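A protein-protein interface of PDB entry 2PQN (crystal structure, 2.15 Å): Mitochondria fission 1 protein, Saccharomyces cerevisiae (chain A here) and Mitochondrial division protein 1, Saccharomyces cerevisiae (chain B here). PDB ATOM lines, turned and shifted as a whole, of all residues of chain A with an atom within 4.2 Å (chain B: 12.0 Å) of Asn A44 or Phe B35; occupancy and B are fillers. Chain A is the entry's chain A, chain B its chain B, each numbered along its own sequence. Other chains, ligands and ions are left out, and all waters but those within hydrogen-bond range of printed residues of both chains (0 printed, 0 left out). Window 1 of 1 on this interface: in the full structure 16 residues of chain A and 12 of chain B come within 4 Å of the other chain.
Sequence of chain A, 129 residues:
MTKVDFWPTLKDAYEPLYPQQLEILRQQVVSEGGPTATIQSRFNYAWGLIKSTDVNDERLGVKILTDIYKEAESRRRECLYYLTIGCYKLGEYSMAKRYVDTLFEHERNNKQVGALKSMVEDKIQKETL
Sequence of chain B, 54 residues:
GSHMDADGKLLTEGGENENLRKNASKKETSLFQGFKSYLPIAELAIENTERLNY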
ATOM      1  N   LEU A  25     -34.803  -8.098  10.836  1.00  0.00           N
ATOM      2  CA  LEU A  25     -33.354  -8.026  10.892  1.00  0.00           C
ATOM      3  C   LEU A  25     -32.886  -7.682  12.320  1.00  0.00           C
ATOM      4  O   LEU A  25     -31.833  -8.158  12.800  1.00  0.00           O
ATOM      5  CB  LEU A  25     -32.855  -6.976   9.878  1.00  0.00           C
ATOM      6  CG  LEU A  25     -33.135  -7.151   8.415  1.00  0.00           C
ATOM      7  CD1 LEU A  25     -32.588  -5.977   7.719  1.00  0.00           C
ATOM      8  CD2 LEU A  25     -32.458  -8.421   7.938  1.00  0.00           C
ATOM      9  N   GLN A  40     -22.377 -11.497   9.870  1.00  0.00           N
ATOM     10  CA  GLN A  40     -23.449 -11.458   8.853  1.00  0.00           C
ATOM     11  C   GLN A  40     -24.734 -10.825   9.385  1.00  0.00           C
ATOM     12  O   GLN A  40     -25.216  -9.852   8.806  1.00  0.00           O
ATOM     13  CB  GLN A  40     -23.707 -12.864   8.231  1.00  0.00           C
ATOM     14  CG  GLN A  40     -24.609 -12.846   6.975  1.00  0.00           C
ATOM     15  CD  GLN A  40     -24.015 -12.026   5.840  1.00  0.00           C
ATOM     16  OE1 GLN A  40     -22.965 -12.370   5.308  1.00  0.00           O
ATOM     17  NE2 GLN A  40     -24.665 -10.917   5.489  1.00  0.00           N
ATOM     18  N   SER A  41     -25.252 -11.340  10.510  1.00  0.00           N
ATOM     19  CA  SER A  41     -26.544 -10.861  11.030  1.00  0.00           C
ATOM     20  C   SER A  41     -26.505  -9.367  11.420  1.00  0.00           C
ATOM     21  O   SER A  41     -27.471  -8.613  11.190  1.00  0.00           O
ATOM     22  CB  SER A  41     -26.993 -11.694  12.220  1.00  0.00           C
ATOM     23  OG  SER A  41     -27.070 -13.060  11.837  1.00  0.00           O
ATOM     24  N   ARG A  42     -25.371  -8.969  11.981  1.00  0.00           N
ATOM     25  CA  ARG A  42     -25.111  -7.576  12.323  1.00  0.00           C
ATOM     26  C   ARG A  42     -24.978  -6.701  11.079  1.00  0.00           C
ATOM     27  O   ARG A  42     -25.512  -5.578  11.062  1.00  0.00           O
ATOM     28  CB  ARG A  42     -23.853  -7.473  13.198  1.00  0.00           C
ATOM     29  CG  ARG A  42     -24.131  -7.789  14.663  1.00  0.00           C
ATOM     30  CD  ARG A  42     -22.923  -7.481  15.572  1.00  0.00           C
ATOM     31  NE  ARG A  42     -21.875  -8.467  15.351  1.00  0.00           N
ATOM     32  CZ  ARG A  42     -20.588  -8.196  15.147  1.00  0.00           C
ATOM     33  NH1 ARG A  42     -20.136  -6.947  15.166  1.00  0.00           N
ATOM     34  NH2 ARG A  42     -19.743  -9.191  14.938  1.00  0.00           N
ATOM     35  N   PHE A  43     -24.262  -7.183  10.064  1.00  0.00           N
ATOM     36  CA  PHE A  43     -24.190  -6.425   8.802  1.00  0.00           C
ATOM     37  C   PHE A  43     -25.557  -6.248   8.219  1.00  0.00           C
ATOM     38  O   PHE A  43     -25.909  -5.162   7.782  1.00  0.00           O
ATOM     39  CB  PHE A  43     -23.291  -7.050   7.719  1.00  0.00           C
ATOM     40  CG  PHE A  43     -23.555  -6.467   6.322  1.00  0.00           C
ATOM     41  CD1 PHE A  43     -22.861  -5.339   5.871  1.00  0.00           C
ATOM     42  CD2 PHE A  43     -24.542  -7.016   5.482  1.00  0.00           C
ATOM     43  CE1 PHE A  43     -23.130  -4.787   4.599  1.00  0.00           C
ATOM     44  CE2 PHE A  43     -24.802  -6.469   4.196  1.00  0.00           C
ATOM     45  CZ  PHE A  43     -24.105  -5.351   3.770  1.00  0.00           C
ATOM     46  N   ASN A  44     -26.321  -7.335   8.173  1.00  0.00           N
ATOM     47  CA  ASN A  44     -27.667  -7.289   7.612  1.00  0.00           C
ATOM     48  C   ASN A  44     -28.517  -6.186   8.259  1.00  0.00           C
ATOM     49  O   ASN A  44     -29.192  -5.407   7.587  1.00  0.00           O
ATOM     50  CB  ASN A  44     -28.347  -8.624   7.807  1.00  0.00           C
ATOM     51  CG  ASN A  44     -27.798  -9.713   6.884  1.00  0.00           C
ATOM     52  OD1 ASN A  44     -28.214 -10.867   7.000  1.00  0.00           O
ATOM     53  ND2 ASN A  44     -26.861  -9.373   5.997  1.00  0.00           N
ATOM     54  N   TYR A  45     -28.494  -6.145   9.575  1.00  0.00           N
ATOM     55  CA  TYR A  45     -29.265  -5.157  10.299  1.00  0.00           C
ATOM     56  C   TYR A  45     -28.682  -3.752  10.029  1.00  0.00           C
ATOM     57  O   TYR A  45     -29.413  -2.819   9.762  1.00  0.00           O
ATOM     58  CB  TYR A  45     -29.294  -5.547  11.769  1.00  0.00           C
ATOM     59  CG  TYR A  45     -30.106  -4.610  12.668  1.00  0.00           C
ATOM     60  CD1 TYR A  45     -31.356  -4.152  12.267  1.00  0.00           C
ATOM     61  CD2 TYR A  45     -29.607  -4.181  13.908  1.00  0.00           C
ATOM     62  CE1 TYR A  45     -32.125  -3.261  13.104  1.00  0.00           C
ATOM     63  CE2 TYR A  45     -30.352  -3.285  14.752  1.00  0.00           C
ATOM     64  CZ  TYR A  45     -31.613  -2.846  14.336  1.00  0.00           C
ATOM     65  OH  TYR A  45     -32.410  -1.998  15.100  1.00  0.00           O
ATOM     66  N   ALA A  46     -27.358  -3.630  10.028  1.00  0.00           N
ATOM     67  CA  ALA A  46     -26.699  -2.347   9.780  1.00  0.00           C
ATOM     68  C   ALA A  46     -27.081  -1.794   8.409  1.00  0.00           C
ATOM     69  O   ALA A  46     -27.339  -0.620   8.275  1.00  0.00           O
ATOM     70  CB  ALA A  46     -25.173  -2.521   9.844  1.00  0.00           C
ATOM     71  N   TRP A  47     -27.075  -2.649   7.382  1.00  0.00           N
ATOM     72  CA  TRP A  47     -27.453  -2.266   6.020  1.00  0.00           C
ATOM     73  C   TRP A  47     -28.922  -1.822   5.974  1.00  0.00           C
ATOM     74  O   TRP A  47     -29.219  -0.805   5.362  1.00  0.00           O
ATOM     75  CB  TRP A  47     -27.143  -3.417   5.007  1.00  0.00           C
ATOM     76  CG  TRP A  47     -27.579  -3.102   3.585  1.00  0.00           C
ATOM     77  CD1 TRP A  47     -28.436  -3.833   2.807  1.00  0.00           C
ATOM     78  CD2 TRP A  47     -27.194  -1.965   2.781  1.00  0.00           C
ATOM     79  NE1 TRP A  47     -28.601  -3.240   1.584  1.00  0.00           N
ATOM     80  CE2 TRP A  47     -27.877  -2.070   1.559  1.00  0.00           C
ATOM     81  CE3 TRP A  47     -26.374  -0.850   3.003  1.00  0.00           C
ATOM     82  CZ2 TRP A  47     -27.743  -1.120   0.540  1.00  0.00           C
ATOM     83  CZ3 TRP A  47     -26.247   0.095   1.990  1.00  0.00           C
ATOM     84  CH2 TRP A  47     -26.923  -0.047   0.783  1.00  0.00           C
ATOM     85  N   GLY A  48     -29.857  -2.555   6.604  1.00  0.00           N
ATOM     86  CA  GLY A  48     -31.216  -2.037   6.716  1.00  0.00           C
ATOM     87  C   GLY A  48     -31.355  -0.687   7.462  1.00  0.00           C
ATOM     88  O   GLY A  48     -32.170   0.166   7.078  1.00  0.00           O
ATOM     89  N   GLU B  28     -14.357 -14.368  -1.344  1.00  0.00           N
ATOM     90  CA  GLU B  28     -15.464 -14.914  -0.474  1.00  0.00           C
ATOM     91  C   GLU B  28     -16.775 -14.204  -0.798  1.00  0.00           C
ATOM     92  O   GLU B  28     -16.779 -12.995  -1.151  1.00  0.00           O
ATOM     93  CB  GLU B  28     -15.133 -14.777   1.033  1.00  0.00           C
ATOM     94  CG  GLU B  28     -13.635 -15.019   1.402  1.00  0.00           C
ATOM     95  CD  GLU B  28     -12.900 -15.923   0.389  1.00  0.00           C
ATOM     96  OE1 GLU B  28     -11.982 -15.414  -0.313  1.00  0.00           O
ATOM     97  OE2 GLU B  28     -13.270 -17.123   0.269  1.00  0.00           O
ATOM     98  N   THR B  29     -17.872 -14.961  -0.687  1.00  0.00           N
ATOM     99  CA  THR B  29     -19.216 -14.462  -0.991  1.00  0.00           C
ATOM    100  C   THR B  29     -19.533 -13.255  -0.108  1.00  0.00           C
ATOM    101  O   THR B  29     -19.283 -13.275   1.097  1.00  0.00           O
ATOM    102  CB  THR B  29     -20.297 -15.597  -0.957  1.00  0.00           C
ATOM    103  OG1 THR B  29     -21.535 -15.100  -0.444  1.00  0.00           O
ATOM    104  CG2 THR B  29     -19.838 -16.790  -0.120  1.00  0.00           C
ATOM    105  N   SER B  30     -20.017 -12.186  -0.730  1.00  0.00           N
ATOM    106  CA  SER B  30     -20.129 -10.894  -0.053  1.00  0.00           C
ATOM    107  C   SER B  30     -21.170 -10.845   1.063  1.00  0.00           C
ATOM    108  O   SER B  30     -22.128 -11.607   1.088  1.00  0.00           O
ATOM    109  CB  SER B  30     -20.432  -9.777  -1.057  1.00  0.00           C
ATOM    110  OG  SER B  30     -21.798  -9.809  -1.432  1.00  0.00           O
ATOM    111  N   LEU B  31     -20.967  -9.899   1.974  1.00  0.00           N
ATOM    112  CA  LEU B  31     -21.988  -9.544   2.967  1.00  0.00           C
ATOM    113  C   LEU B  31     -23.308  -9.204   2.294  1.00  0.00           C
ATOM    114  O   LEU B  31     -24.357  -9.684   2.732  1.00  0.00           O
ATOM    115  CB  LEU B  31     -21.518  -8.368   3.794  1.00  0.00           C
ATOM    116  CG  LEU B  31     -20.272  -8.670   4.605  1.00  0.00           C
ATOM    117  CD1 LEU B  31     -19.700  -7.382   5.183  1.00  0.00           C
ATOM    118  CD2 LEU B  31     -20.596  -9.692   5.672  1.00  0.00           C
ATOM    119  N   PHE B  32     -23.257  -8.414   1.216  1.00  0.00           N
ATOM    120  CA  PHE B  32     -24.478  -8.013   0.523  1.00  0.00           C
ATOM    121  C   PHE B  32     -25.219  -9.230  -0.024  1.00  0.00           C
ATOM    122  O   PHE B  32     -26.442  -9.303   0.067  1.00  0.00           O
ATOM    123  CB  PHE B  32     -24.186  -6.976  -0.559  1.00  0.00           C
ATOM    124  CG  PHE B  32     -25.408  -6.539  -1.362  1.00  0.00           C
ATOM    125  CD1 PHE B  32     -26.534  -5.997  -0.733  1.00  0.00           C
ATOM    126  CD2 PHE B  32     -25.406  -6.635  -2.756  1.00  0.00           C
ATOM    127  CE1 PHE B  32     -27.641  -5.570  -1.478  1.00  0.00           C
ATOM    128  CE2 PHE B  32     -26.517  -6.220  -3.517  1.00  0.00           C
ATOM    129  CZ  PHE B  32     -27.637  -5.697  -2.877  1.00  0.00           C
ATOM    130  N   GLN B  33     -24.452 -10.198  -0.560  1.00  0.00           N
ATOM    131  CA  GLN B  33     -25.022 -11.435  -1.094  1.00  0.00           C
ATOM    132  C   GLN B  33     -25.696 -12.221   0.021  1.00  0.00           C
ATOM    133  O   GLN B  33     -26.837 -12.674  -0.149  1.00  0.00           O
ATOM    134  CB  GLN B  33     -23.977 -12.250  -1.867  1.00  0.00           C
ATOM    135  CG  GLN B  33     -23.446 -11.469  -3.103  1.00  0.00           C
ATOM    136  CD  GLN B  33     -22.352 -12.204  -3.920  1.00  0.00           C
ATOM    137  OE1 GLN B  33     -21.365 -11.584  -4.381  1.00  0.00           O
ATOM    138  NE2 GLN B  33     -22.547 -13.521  -4.132  1.00  0.00           N
ATOM    139  N   GLY B  34     -25.040 -12.330   1.181  1.00  0.00           N
ATOM    140  CA  GLY B  34     -25.704 -12.938   2.319  1.00  0.00           C
ATOM    141  C   GLY B  34     -26.952 -12.179   2.757  1.00  0.00           C
ATOM    142  O   GLY B  34     -27.942 -12.767   3.214  1.00  0.00           O
ATOM    143  N   PHE B  35     -26.941 -10.862   2.627  1.00  0.00           N
ATOM    144  CA  PHE B  35     -28.120 -10.115   3.017  1.00  0.00           C
ATOM    145  C   PHE B  35     -29.268 -10.440   2.045  1.00  0.00           C
ATOM    146  O   PHE B  35     -30.414 -10.663   2.458  1.00  0.00           O
ATOM    147  CB  PHE B  35     -27.812  -8.608   3.034  1.00  0.00           C
ATOM    148  CG  PHE B  35     -29.031  -7.730   3.020  1.00  0.00           C
ATOM    149  CD1 PHE B  35     -29.677  -7.391   4.218  1.00  0.00           C
ATOM    150  CD2 PHE B  35     -29.522  -7.240   1.817  1.00  0.00           C
ATOM    151  CE1 PHE B  35     -30.813  -6.573   4.193  1.00  0.00           C
ATOM    152  CE2 PHE B  35     -30.652  -6.481   1.758  1.00  0.00           C
ATOM    153  CZ  PHE B  35     -31.306  -6.107   2.936  1.00  0.00           C
ATOM    154  N   LYS B  36     -28.982 -10.390   0.756  1.00  0.00           N
ATOM    155  CA  LYS B  36     -30.056 -10.643  -0.220  1.00  0.00           C
ATOM    156  C   LYS B  36     -30.668 -12.053  -0.095  1.00  0.00           C
ATOM    157  O   LYS B  36     -31.851 -12.178  -0.315  1.00  0.00           O
ATOM    158  CB  LYS B  36     -29.661 -10.300  -1.668  1.00  0.00           C
ATOM    159  CG  LYS B  36     -29.334  -8.795  -1.861  1.00  0.00           C
ATOM    160  CD  LYS B  36     -30.563  -7.799  -1.846  1.00  0.00           C
ATOM    161  CE  LYS B  36     -31.433  -7.923  -3.112  1.00  0.00           C
ATOM    162  NZ  LYS B  36     -31.640  -6.597  -3.768  1.00  0.00           N
ATOM    163  N   SER B  37     -29.895 -13.051   0.324  1.00  0.00           N
ATOM    164  CA  SER B  37     -30.442 -14.364   0.692  1.00  0.00           C
ATOM    165  C   SER B  37     -31.343 -14.391   1.908  1.00  0.00           C
ATOM    166  O   SER B  37     -32.386 -15.094   1.884  1.00  0.00           O
ATOM    167  CB  SER B  37     -29.352 -15.395   0.917  1.00  0.00           C
ATOM    168  OG  SER B  37     -28.573 -15.554  -0.240  1.00  0.00           O
ATOM    169  N   TYR B  38     -30.960 -13.630   2.955  1.00  0.00           N
ATOM    170  CA  TYR B  38     -31.594 -13.743   4.258  1.00  0.00           C
ATOM    171  C   TYR B  38     -33.073 -13.368   4.220  1.00  0.00           C
ATOM    172  O   TYR B  38     -33.901 -14.121   4.752  1.00  0.00           O
ATOM    173  CB  TYR B  38     -30.846 -12.922   5.369  1.00  0.00           C
ATOM    174  CG  TYR B  38     -31.559 -12.991   6.714  1.00  0.00           C
ATOM    175  CD1 TYR B  38     -31.394 -14.094   7.532  1.00  0.00           C
ATOM    176  CD2 TYR B  38     -32.451 -11.972   7.137  1.00  0.00           C
ATOM    177  CE1 TYR B  38     -32.066 -14.199   8.752  1.00  0.00           C
ATOM    178  CE2 TYR B  38     -33.126 -12.063   8.412  1.00  0.00           C
ATOM    179  CZ  TYR B  38     -32.926 -13.185   9.179  1.00  0.00           C
ATOM    180  OH  TYR B  38     -33.560 -13.368  10.371  1.00  0.00           O
ATOM    181  N   LEU B  39     -33.419 -12.211   3.662  1.00  0.00           N
ATOM    182  CA  LEU B  39     -34.770 -11.674   3.885  1.00  0.00           C
ATOM    183  C   LEU B  39     -35.909 -12.423   3.201  1.00  0.00           C
ATOM    184  O   LEU B  39     -37.003 -12.518   3.778  1.00  0.00           O
ATOM    185  CB  LEU B  39     -34.889 -10.178   3.537  1.00  0.00           C
ATOM    186  CG  LEU B  39     -34.927  -9.122   4.660  1.00  0.00           C
ATOM    187  CD1 LEU B  39     -35.081  -7.763   4.041  1.00  0.00           C
ATOM    188  CD2 LEU B  39     -36.035  -9.353   5.725  1.00  0.00           C
ATOM    189  N   PRO B  40     -35.711 -12.880   1.933  1.00  0.00           N
ATOM    190  CA  PRO B  40     -36.797 -13.678   1.366  1.00  0.00           C
ATOM    191  C   PRO B  40     -37.151 -14.907   2.171  1.00  0.00           C
ATOM    192  O   PRO B  40     -38.326 -15.251   2.288  1.00  0.00           O
ATOM    193  CB  PRO B  40     -36.279 -14.036  -0.047  1.00  0.00           C
ATOM    194  CG  PRO B  40     -35.345 -12.933  -0.387  1.00  0.00           C
ATOM    195  CD  PRO B  40     -34.645 -12.629   0.944  1.00  0.00           C
ATOM    196  N   ILE B  41     -36.138 -15.550   2.734  1.00  0.00           N
ATOM    197  CA  ILE B  41     -36.330 -16.789   3.498  1.00  0.00           C
ATOM    198  C   ILE B  41     -36.959 -16.517   4.849  1.00  0.00           C
ATOM    199  O   ILE B  41     -37.875 -17.233   5.265  1.00  0.00           O
ATOM    200  CB  ILE B  41     -35.018 -17.572   3.627  1.00  0.00           C
ATOM    201  CG1 ILE B  41     -34.473 -17.978   2.231  1.00  0.00           C
ATOM    202  CG2 ILE B  41     -35.189 -18.807   4.500  1.00  0.00           C
ATOM    203  CD1 ILE B  41     -35.518 -18.632   1.275  1.00  0.00           C
ATOM    204  N   ALA B  42     -36.485 -15.458   5.520  1.00  0.00           N
ATOM    205  CA  ALA B  42     -37.111 -14.974   6.751  1.00  0.00           C
ATOM    206  C   ALA B  42     -38.582 -14.619   6.569  1.00  0.00           C
ATOM    207  O   ALA B  42     -39.419 -14.968   7.389  1.00  0.00           O
ATOM    208  CB  ALA B  42     -36.308 -13.798   7.364  1.00  0.00           C
ATOM    209  N   GLU B  43     -38.920 -13.966   5.473  1.00  0.00           N
ATOM    210  CA  GLU B  43     -40.328 -13.666   5.191  1.00  0.00           C
ATOM    211  C   GLU B  43     -41.172 -14.908   4.885  1.00  0.00           C
ATOM    212  O   GLU B  43     -42.376 -14.935   5.125  1.00  0.00           O
ATOM    213  CB  GLU B  43     -40.424 -12.669   4.044  1.00  0.00           C
ATOM    214  CG  GLU B  43     -39.825 -11.293   4.404  1.00  0.00           C
ATOM    215  CD  GLU B  43     -39.763 -10.334   3.214  1.00  0.00           C
ATOM    216  OE1 GLU B  43     -39.433 -10.770   2.073  1.00  0.00           O
ATOM    217  OE2 GLU B  43     -40.046  -9.146   3.417  1.00  0.00           O
ATOM    218  N   LEU B  44     -40.520 -15.948   4.369  1.00  0.00           N
ATOM    219  CA  LEU B  44     -41.168 -17.204   4.082  1.00  0.00           C
ATOM    220  C   LEU B  44     -41.591 -17.854   5.411  1.00  0.00           C
ATOM    221  O   LEU B  44     -42.657 -18.477   5.529  1.00  0.00           O
ATOM    222  CB  LEU B  44     -40.173 -18.084   3.276  1.00  0.00           C
ATOM    223  CG  LEU B  44     -40.539 -19.489   2.877  1.00  0.00           C
ATOM    224  CD1 LEU B  44     -41.651 -19.356   1.855  1.00  0.00           C
ATOM    225  CD2 LEU B  44     -39.306 -20.306   2.336  1.00  0.00           C
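The backbone carbonyl oxygen of Leu B31 sits at hydrogen-bond distance from the side-chain amide nitrogen of Gln A40, 3.0 Å away.
The side-chain amide nitrogen of Gln A40 lies close to the side-chain amide nitrogen of Asn A44, 2.7 Å away. N of Phe B32 sits close to OG of Ser B30, at 3.3 Å.
Among the printed residues, merely in contact across the chains: Leu A25 with Phe B35, Leu A25 with Tyr B38, Gln A40 with Gly B34, Gln A40 with Phe B35, Phe A43 with Leu B31, Phe A43 with Phe B32, Phe A43 with Phe B35, Asn A44 with Phe B35, Asn A44 with Tyr B38, Trp A47 with Phe B32 and Trp A47 with Phe B35.
Asn A44 touches just these residues of chain B: Phe B35 (3.2 Å) and Tyr B38 (3.7 Å). Printed residues of chain A within 4 Å of Phe B35: Leu A25, Gln A40, Phe A43, Asn A44 and Trp A47. Of chain B, only Leu B31, Gly B34 and Phe B35 come within 4 Å of Gln A40. No residue of chain B comes within 4 Å of Ser A41. Phe A43 touches three residues of chain B. No residue of chain B comes within 4 Å of Ala A46. Printed residues of chain A within 4 Å of Leu B31: Gln A40 and Phe A43. Of the printed residues of chain A, Tyr B38 touches Leu A25 (3.6 Å) and Asn A44 (3.7 Å). Printed residues of chain A within 4 Å of Gly B34: Gln A40. Of the printed residues of chain B, Leu A25 touches Phe B35 (3.99 Å) and Tyr B38 (3.6 Å). Printed residues of chain A within 4 Å of Phe B32: Phe A43 (3.9 Å) and Trp A47 (3.97 Å). Pro B40 touches none of the printed residues of chain A. The nearest printed residue of chain A that does not touch Phe B35 is Gly A48 (4.8 Å).
Of the 17 printed residues of chain B, 5 touch a printed residue of chain A. Hydrophobic or aromatic side chains of chain B within 4 Å of the printed part of chain A: Leu B31, Phe B32, Phe B35 and Tyr B38. Along chain A the printed residues that touch a printed residue of chain B span positions 25 to 47. Among the printed residues, 12 pairs touch across the chains.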
